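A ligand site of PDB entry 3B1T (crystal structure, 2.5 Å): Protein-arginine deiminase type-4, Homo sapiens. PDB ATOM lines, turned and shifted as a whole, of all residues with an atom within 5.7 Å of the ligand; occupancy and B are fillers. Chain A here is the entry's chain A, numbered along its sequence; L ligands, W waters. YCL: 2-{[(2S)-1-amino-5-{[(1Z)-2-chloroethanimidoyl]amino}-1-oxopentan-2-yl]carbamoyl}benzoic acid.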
ATOM      1  N   ASP A 352      21.462  -1.204 -20.912  1.00  0.00           N
ATOM      2  CA  ASP A 352      22.066   0.047 -21.402  1.00  0.00           C
ATOM      3  C   ASP A 352      21.516   1.331 -20.734  1.00  0.00           C
ATOM      4  O   ASP A 352      21.746   2.446 -21.220  1.00  0.00           O
ATOM      5  CB  ASP A 352      22.045   0.118 -22.950  1.00  0.00           C
ATOM      6  CG  ASP A 352      23.439  -0.040 -23.569  1.00  0.00           C
ATOM      7  OD1 ASP A 352      23.750  -1.126 -24.130  1.00  0.00           O
ATOM      8  OD2 ASP A 352      24.239   0.924 -23.470  1.00  0.00           O
ATOM      9  N   GLN A 354      21.817   3.983 -17.993  1.00  0.00           N
ATOM     10  CA  GLN A 354      22.899   4.560 -17.187  1.00  0.00           C
ATOM     11  C   GLN A 354      22.460   5.427 -15.987  1.00  0.00           C
ATOM     12  O   GLN A 354      23.314   5.827 -15.185  1.00  0.00           O
ATOM     13  CB  GLN A 354      23.831   5.365 -18.095  1.00  0.00           C
ATOM     14  CG  GLN A 354      23.241   6.676 -18.597  1.00  0.00           C
ATOM     15  CD  GLN A 354      23.949   7.203 -19.810  1.00  0.00           C
ATOM     16  OE1 GLN A 354      23.399   7.186 -20.906  1.00  0.00           O
ATOM     17  NE2 GLN A 354      25.173   7.665 -19.630  1.00  0.00           N
ATOM     18  N   TRP A 355      21.164   5.709 -15.846  1.00  0.00           N
ATOM     19  CA  TRP A 355      20.715   6.809 -14.944  1.00  0.00           C
ATOM     20  C   TRP A 355      20.331   6.357 -13.542  1.00  0.00           C
ATOM     21  O   TRP A 355      19.157   6.366 -13.168  1.00  0.00           O
ATOM     22  CB  TRP A 355      19.581   7.578 -15.610  1.00  0.00           C
ATOM     23  CG  TRP A 355      19.996   8.087 -16.935  1.00  0.00           C
ATOM     24  CD1 TRP A 355      19.550   7.664 -18.158  1.00  0.00           C
ATOM     25  CD2 TRP A 355      21.000   9.077 -17.201  1.00  0.00           C
ATOM     26  NE1 TRP A 355      20.198   8.350 -19.167  1.00  0.00           N
ATOM     27  CE2 TRP A 355      21.091   9.224 -18.606  1.00  0.00           C
ATOM     28  CE3 TRP A 355      21.815   9.863 -16.380  1.00  0.00           C
ATOM     29  CZ2 TRP A 355      21.970  10.138 -19.207  1.00  0.00           C
ATOM     30  CZ3 TRP A 355      22.699  10.761 -16.982  1.00  0.00           C
ATOM     31  CH2 TRP A 355      22.764  10.893 -18.382  1.00  0.00           C
ATOM     32  N   GLN A 357      20.440   7.458 -10.595  1.00  0.00           N
ATOM     33  CA  GLN A 357      19.716   8.405  -9.782  1.00  0.00           C
ATOM     34  C   GLN A 357      18.201   8.302  -9.942  1.00  0.00           C
ATOM     35  O   GLN A 357      17.432   8.609  -9.017  1.00  0.00           O
ATOM     36  CB  GLN A 357      20.155   9.823 -10.189  1.00  0.00           C
ATOM     37  CG  GLN A 357      19.433  11.002  -9.533  1.00  0.00           C
ATOM     38  CD  GLN A 357      19.390  10.935  -8.034  1.00  0.00           C
ATOM     39  OE1 GLN A 357      18.392  11.328  -7.439  1.00  0.00           O
ATOM     40  NE2 GLN A 357      20.467  10.467  -7.407  1.00  0.00           N
ATOM     41  N   ASP A 358      17.778   7.882 -11.122  1.00  0.00           N
ATOM     42  CA  ASP A 358      16.385   8.023 -11.520  1.00  0.00           C
ATOM     43  C   ASP A 358      15.437   6.880 -11.097  1.00  0.00           C
ATOM     44  O   ASP A 358      14.291   7.160 -10.763  1.00  0.00           O
ATOM     45  CB  ASP A 358      16.314   8.227 -13.030  1.00  0.00           C
ATOM     46  CG  ASP A 358      16.994   9.515 -13.465  1.00  0.00           C
ATOM     47  OD1 ASP A 358      17.298  10.381 -12.616  1.00  0.00           O
ATOM     48  OD2 ASP A 358      17.217   9.667 -14.677  1.00  0.00           O
ATOM     49  N   ARG A 380       9.211   4.498 -13.199  1.00  0.00           N
ATOM     50  CA  ARG A 380       9.675   4.871 -14.522  1.00  0.00           C
ATOM     51  C   ARG A 380      10.036   3.629 -15.352  1.00  0.00           C
ATOM     52  O   ARG A 380       9.898   3.650 -16.581  1.00  0.00           O
ATOM     53  CB  ARG A 380      10.803   5.932 -14.474  1.00  0.00           C
ATOM     54  CG  ARG A 380      12.182   5.439 -14.186  1.00  0.00           C
ATOM     55  CD  ARG A 380      13.228   6.080 -15.114  1.00  0.00           C
ATOM     56  NE  ARG A 380      14.438   5.258 -15.184  1.00  0.00           N
ATOM     57  CZ  ARG A 380      15.621   5.659 -15.648  1.00  0.00           C
ATOM     58  NH1 ARG A 380      15.807   6.892 -16.111  1.00  0.00           N
ATOM     59  NH2 ARG A 380      16.619   4.797 -15.640  1.00  0.00           N
ATOM     60  N   ARG A 382      12.560   1.683 -16.547  1.00  0.00           N
ATOM     61  CA  ARG A 382      13.415   1.798 -17.724  1.00  0.00           C
ATOM     62  C   ARG A 382      14.340   0.564 -17.728  1.00  0.00           C
ATOM     63  O   ARG A 382      13.948  -0.497 -17.240  1.00  0.00           O
ATOM     64  CB  ARG A 382      14.163   3.141 -17.649  1.00  0.00           C
ATOM     65  CG  ARG A 382      14.409   3.836 -18.982  1.00  0.00           C
ATOM     66  CD  ARG A 382      13.333   4.860 -19.382  1.00  0.00           C
ATOM     67  NE  ARG A 382      13.690   6.254 -19.082  1.00  0.00           N
ATOM     68  CZ  ARG A 382      14.614   6.991 -19.712  1.00  0.00           C
ATOM     69  NH1 ARG A 382      15.359   6.488 -20.697  1.00  0.00           N
ATOM     70  NH2 ARG A 382      14.822   8.249 -19.341  1.00  0.00           N
ATOM     71  N   SER A 414      10.842  10.376 -12.393  1.00  0.00           N
ATOM     72  CA  SER A 414      12.179   9.882 -12.105  1.00  0.00           C
ATOM     73  C   SER A 414      12.719  10.553 -10.830  1.00  0.00           C
ATOM     74  O   SER A 414      12.356  11.686 -10.500  1.00  0.00           O
ATOM     75  CB  SER A 414      13.104  10.176 -13.286  1.00  0.00           C
ATOM     76  OG  SER A 414      12.708   9.461 -14.464  1.00  0.00           O
ATOM     77  N   GLY A 416      15.570  11.639  -9.760  1.00  0.00           N
ATOM     78  CA  GLY A 416      16.327  12.886  -9.794  1.00  0.00           C
ATOM     79  C   GLY A 416      15.440  14.060  -9.453  1.00  0.00           C
ATOM     80  O   GLY A 416      15.935  15.142  -9.115  1.00  0.00           O
ATOM     81  N   ASN A 417      14.127  13.834  -9.585  1.00  0.00           N
ATOM     82  CA  ASN A 417      13.117  14.797  -9.188  1.00  0.00           C
ATOM     83  C   ASN A 417      12.586  14.536  -7.777  1.00  0.00           C
ATOM     84  O   ASN A 417      11.497  15.015  -7.445  1.00  0.00           O
ATOM     85  CB  ASN A 417      11.914  14.777 -10.151  1.00  0.00           C
ATOM     86  CG  ASN A 417      11.191  16.113 -10.206  1.00  0.00           C
ATOM     87  OD1 ASN A 417      11.817  17.149  -9.997  1.00  0.00           O
ATOM     88  ND2 ASN A 417       9.894  16.095 -10.454  1.00  0.00           N
ATOM     89  N   VAL A 477      14.624  17.842 -19.046  1.00  0.00           N
ATOM     90  CA  VAL A 477      14.496  16.580 -18.316  1.00  0.00           C
ATOM     91  C   VAL A 477      13.474  16.721 -17.175  1.00  0.00           C
ATOM     92  O   VAL A 477      12.629  15.834 -16.983  1.00  0.00           O
ATOM     93  CB  VAL A 477      15.871  16.066 -17.787  1.00  0.00           C
ATOM     94  CG1 VAL A 477      15.691  14.830 -16.907  1.00  0.00           C
ATOM     95  CG2 VAL A 477      16.816  15.759 -18.944  1.00  0.00           C
ATOM     96  N   HIS A 479      14.087  17.819 -13.624  1.00  0.00           N
ATOM     97  CA  HIS A 479      14.440  17.363 -12.282  1.00  0.00           C
ATOM     98  C   HIS A 479      15.033  18.460 -11.423  1.00  0.00           C
ATOM     99  O   HIS A 479      15.943  19.177 -11.877  1.00  0.00           O
ATOM    100  CB  HIS A 479      15.484  16.268 -12.365  1.00  0.00           C
ATOM    101  CG  HIS A 479      15.027  15.034 -13.050  1.00  0.00           C
ATOM    102  ND1 HIS A 479      15.752  13.865 -13.023  1.00  0.00           N
ATOM    103  CD2 HIS A 479      13.913  14.767 -13.779  1.00  0.00           C
ATOM    104  CE1 HIS A 479      15.126  12.944 -13.726  1.00  0.00           C
ATOM    105  NE2 HIS A 479      14.008  13.470 -14.192  1.00  0.00           N
ATOM    106  N   ASP A 481      17.309  18.196  -9.233  1.00  0.00           N
ATOM    107  CA  ASP A 481      18.779  18.072  -9.052  1.00  0.00           C
ATOM    108  C   ASP A 481      19.518  18.781 -10.156  1.00  0.00           C
ATOM    109  O   ASP A 481      20.708  19.021 -10.053  1.00  0.00           O
ATOM    110  CB  ASP A 481      19.298  16.622  -8.812  1.00  0.00           C
ATOM    111  CG  ASP A 481      19.071  15.658 -10.009  1.00  0.00           C
ATOM    112  OD1 ASP A 481      19.650  14.524  -9.995  1.00  0.00           O
ATOM    113  OD2 ASP A 481      18.339  16.003 -10.962  1.00  0.00           O
ATOM    114  N   GLU A 482      18.778  19.138 -11.207  1.00  0.00           N
ATOM    115  CA  GLU A 482      19.340  19.947 -12.262  1.00  0.00           C
ATOM    116  C   GLU A 482      19.608  21.381 -11.824  1.00  0.00           C
ATOM    117  O   GLU A 482      20.438  22.028 -12.436  1.00  0.00           O
ATOM    118  CB  GLU A 482      18.447  19.953 -13.503  1.00  0.00           C
ATOM    119  CG  GLU A 482      18.268  18.634 -14.121  1.00  0.00           C
ATOM    120  CD  GLU A 482      17.475  18.688 -15.427  1.00  0.00           C
ATOM    121  OE1 GLU A 482      18.048  19.058 -16.479  1.00  0.00           O
ATOM    122  OE2 GLU A 482      16.268  18.329 -15.406  1.00  0.00           O
ATOM    123  N   ASN A 596      24.757  19.651 -10.341  1.00  0.00           N
ATOM    124  CA  ASN A 596      24.352  18.258 -10.330  1.00  0.00           C
ATOM    125  C   ASN A 596      25.541  17.352  -9.910  1.00  0.00           C
ATOM    126  O   ASN A 596      26.151  16.662 -10.737  1.00  0.00           O
ATOM    127  CB  ASN A 596      23.810  17.936 -11.723  1.00  0.00           C
ATOM    128  CG  ASN A 596      23.201  16.568 -11.804  1.00  0.00           C
ATOM    129  OD1 ASN A 596      23.899  15.616 -12.149  1.00  0.00           O
ATOM    130  ND2 ASN A 596      21.922  16.450 -11.458  1.00  0.00           N
ATOM    131  N   ILE A 646      26.007  14.715 -22.912  1.00  0.00           N
ATOM    132  CA  ILE A 646      25.367  14.786 -24.236  1.00  0.00           C
ATOM    133  C   ILE A 646      24.070  13.977 -24.278  1.00  0.00           C
ATOM    134  O   ILE A 646      23.287  14.105 -25.216  1.00  0.00           O
ATOM    135  CB  ILE A 646      26.316  14.368 -25.424  1.00  0.00           C
ATOM    136  CG1 ILE A 646      26.748  12.887 -25.330  1.00  0.00           C
ATOM    137  CG2 ILE A 646      27.537  15.272 -25.474  1.00  0.00           C
ATOM    138  CD1 ILE A 646      27.463  12.374 -26.587  1.00  0.00           C
ATOM    139  N   ARG A 647      23.870  13.146 -23.255  1.00  0.00           N
ATOM    140  CA  ARG A 647      22.611  12.407 -23.063  1.00  0.00           C
ATOM    141  C   ARG A 647      21.766  13.042 -21.932  1.00  0.00           C
ATOM    142  O   ARG A 647      20.952  12.350 -21.289  1.00  0.00           O
ATOM    143  CB  ARG A 647      22.903  10.912 -22.802  1.00  0.00           C
ATOM    144  CG  ARG A 647      23.126  10.095 -24.072  1.00  0.00           C
ATOM    145  CD  ARG A 647      24.420   9.299 -24.081  1.00  0.00           C
ATOM    146  NE  ARG A 647      24.251   7.873 -23.771  1.00  0.00           N
ATOM    147  CZ  ARG A 647      25.139   6.920 -24.078  1.00  0.00           C
ATOM    148  NH1 ARG A 647      26.277   7.225 -24.715  1.00  0.00           N
ATOM    149  NH2 ARG A 647      24.899   5.658 -23.747  1.00  0.00           N
ATOM    150  N   HIS A 648      21.985  14.342 -21.713  1.00  0.00           N
ATOM    151  CA  HIS A 648      21.088  15.216 -20.938  1.00  0.00           C
ATOM    152  C   HIS A 648      21.125  14.977 -19.419  1.00  0.00           C
ATOM    153  O   HIS A 648      20.151  15.249 -18.734  1.00  0.00           O
ATOM    154  CB  HIS A 648      19.647  15.131 -21.472  1.00  0.00           C
ATOM    155  CG  HIS A 648      19.479  15.541 -22.907  1.00  0.00           C
ATOM    156  ND1 HIS A 648      20.527  15.594 -23.803  1.00  0.00           N
ATOM    157  CD2 HIS A 648      18.375  15.868 -23.611  1.00  0.00           C
ATOM    158  CE1 HIS A 648      20.077  15.970 -24.990  1.00  0.00           C
ATOM    159  NE2 HIS A 648      18.774  16.140 -24.902  1.00  0.00           N
ATOM    160  N   GLY A 649      22.250  14.502 -18.891  1.00  0.00           N
ATOM    161  CA  GLY A 649      22.444  14.291 -17.437  1.00  0.00           C
ATOM    162  C   GLY A 649      23.922  14.370 -17.053  1.00  0.00           C
ATOM    163  O   GLY A 649      24.769  14.480 -17.911  1.00  0.00           O
ATOM    164  N   GLU A 650      24.232  14.322 -15.746  1.00  0.00           N
ATOM    165  CA  GLU A 650      25.606  14.463 -15.252  1.00  0.00           C
ATOM    166  C   GLU A 650      26.000  13.390 -14.191  1.00  0.00           C
ATOM    167  O   GLU A 650      25.491  12.256 -14.251  1.00  0.00           O
ATOM    168  CB  GLU A 650      25.860  15.884 -14.709  1.00  0.00           C
ATOM    169  CG  GLU A 650      25.282  17.056 -15.521  1.00  0.00           C
ATOM    170  CD  GLU A 650      25.905  17.246 -16.901  1.00  0.00           C
ATOM    171  OE1 GLU A 650      25.293  17.972 -17.718  1.00  0.00           O
ATOM    172  OE2 GLU A 650      26.995  16.702 -17.182  1.00  0.00           O
ATOM    173  N   HIS A 652      25.621  13.423 -10.722  1.00  0.00           N
ATOM    174  CA  HIS A 652      24.532  13.124  -9.778  1.00  0.00           C
ATOM    175  C   HIS A 652      23.499  12.217 -10.443  1.00  0.00           C
ATOM    176  O   HIS A 652      22.981  11.305  -9.801  1.00  0.00           O
ATOM    177  CB  HIS A 652      23.869  14.391  -9.234  1.00  0.00           C
ATOM    178  CG  HIS A 652      22.921  14.125  -8.108  1.00  0.00           C
ATOM    179  ND1 HIS A 652      21.555  14.086  -8.281  1.00  0.00           N
ATOM    180  CD2 HIS A 652      23.144  13.880  -6.792  1.00  0.00           C
ATOM    181  CE1 HIS A 652      20.969  13.829  -7.120  1.00  0.00           C
ATOM    182  NE2 HIS A 652      21.913  13.708  -6.194  1.00  0.00           N
ATOM    183  N   CYS A 653      23.269  12.439 -11.726  1.00  0.00           N
ATOM    184  CA  CYS A 653      22.310  11.627 -12.473  1.00  0.00           C
ATOM    185  C   CYS A 653      22.799  10.211 -12.798  1.00  0.00           C
ATOM    186  O   CYS A 653      21.999   9.318 -13.018  1.00  0.00           O
ATOM    187  CB  CYS A 653      21.911  12.320 -13.780  1.00  0.00           C
ATOM    188  SG  CYS A 653      21.484  14.055 -13.645  1.00  0.00           S
HETATM  189  C1  YCL L   1      19.212   7.380 -22.974  1.00  0.00           C
HETATM  190  O1  YCL L   1      18.196   6.659 -23.139  1.00  0.00           O
HETATM  191  O2  YCL L   1      20.189   6.992 -22.292  1.00  0.00           O
HETATM  192  NAA YCL L   1      16.185  12.343 -20.275  1.00  0.00           N
HETATM  193  NAC YCL L   1      18.273  12.862 -13.097  1.00  0.00           N
HETATM  194  OAE YCL L   1      15.476  11.159 -18.531  1.00  0.00           O
HETATM  195  OAF YCL L   1      16.995   9.042 -21.616  1.00  0.00           O
HETATM  196  CAH YCL L   1      19.909  10.071 -25.563  1.00  0.00           C
HETATM  197  CAI YCL L   1      19.863   8.839 -24.893  1.00  0.00           C
HETATM  198  CAJ YCL L   1      19.325  11.195 -24.981  1.00  0.00           C
HETATM  199  CAK YCL L   1      19.244   8.728 -23.641  1.00  0.00           C
HETATM  200  CAL YCL L   1      18.708  11.091 -23.736  1.00  0.00           C
HETATM  201  CAM YCL L   1      18.337  12.403 -17.497  1.00  0.00           C
HETATM  202  CAN YCL L   1      18.427  11.978 -16.028  1.00  0.00           C
HETATM  203  CAO YCL L   1      18.743  11.302 -18.477  1.00  0.00           C
HETATM  204  CAP YCL L   1      19.799  14.660 -13.623  1.00  0.00           C
HETATM  205  NAR YCL L   1      19.080  13.069 -15.310  1.00  0.00           N
HETATM  206  NAS YCL L   1      18.321  10.622 -20.716  1.00  0.00           N
HETATM  207  CAU YCL L   1      16.355  11.397 -19.356  1.00  0.00           C
HETATM  208  CAV YCL L   1      18.990  13.466 -14.033  1.00  0.00           C
HETATM  209  CAW YCL L   1      17.950   9.816 -21.724  1.00  0.00           C
HETATM  210  CAX YCL L   1      18.664   9.865 -23.058  1.00  0.00           C
HETATM  211  CAZ YCL L   1      17.682  10.667 -19.387  1.00  0.00           C
HETATM  212  O   HOH W   1      21.364   5.178 -20.775  1.00  0.00           O
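The side-chain amide nitrogen (ND2) of Asn 596 sits at hydrogen-bond distance from the backbone carbonyl oxygen (O) of Asp 481.
ND1 of His 648 is in hydrogen-bond range of O of Ile 646, at 3.4 Å.
OD1 of Asp 481 sits at hydrogen-bond distance from ND1 of His 652 (2.6 Å).
OD1 of Asn 596 lies within hydrogen-bond range of N of His 652 (3.1 Å).
OE1 of Gln 354 lies within hydrogen-bond range of NE of Arg 647, at 3.1 Å.
O of Gly 416 lies close to N of Asp 481, at 3.4 Å.
N of Glu 650 lies within hydrogen-bond range of SG of Cys 653.
The side-chain sulfur (SG) of Cys 653 lies close to the side-chain amide oxygen (OD1) of Asn 596 (3.2 Å).
The side-chain carboxylate (OD1) of Asp 481 is in salt-bridge range of a nitrogen (NAC) of the ligand (3.8 Å).
The backbone carbonyl oxygen (O) of Arg 647 sits at hydrogen-bond distance from a nitrogen (NAS) of the ligand (3.2 Å).
The side-chain sulfur (SG) of Cys 653 is bonded to a carbon (CAP) of the ligand (1.8 Å).
A nitrogen (NAC) of the ligand is in hydrogen-bond range of a ring nitrogen (ND1) of His 479.
A nitrogen (NAC) of the ligand is in salt-bridge range of the side-chain carboxylate of Asp 358 (2.7 Å).
O1 of the ligand lies within salt-bridge range of NH1 of Arg 382 (3.7 Å).
O2 of the ligand sits close to NE1 of Trp 355.
Merely in contact with the ligand: Gln 354, Gly 416, Val 477, Asn 596 and His 648.
Hydrophobic or aromatic side chains that line the ligand: Trp 355, Val 477 and His 479.
The nearest printed residue that does not touch the ligand is Gly 649 (4.2 Å).
Water W1 lies within hydrogen-bond range of an oxygen (O2) of the ligand, the backbone carbonyl oxygen of Asp 352 and the side-chain amide oxygen of Gln 354.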
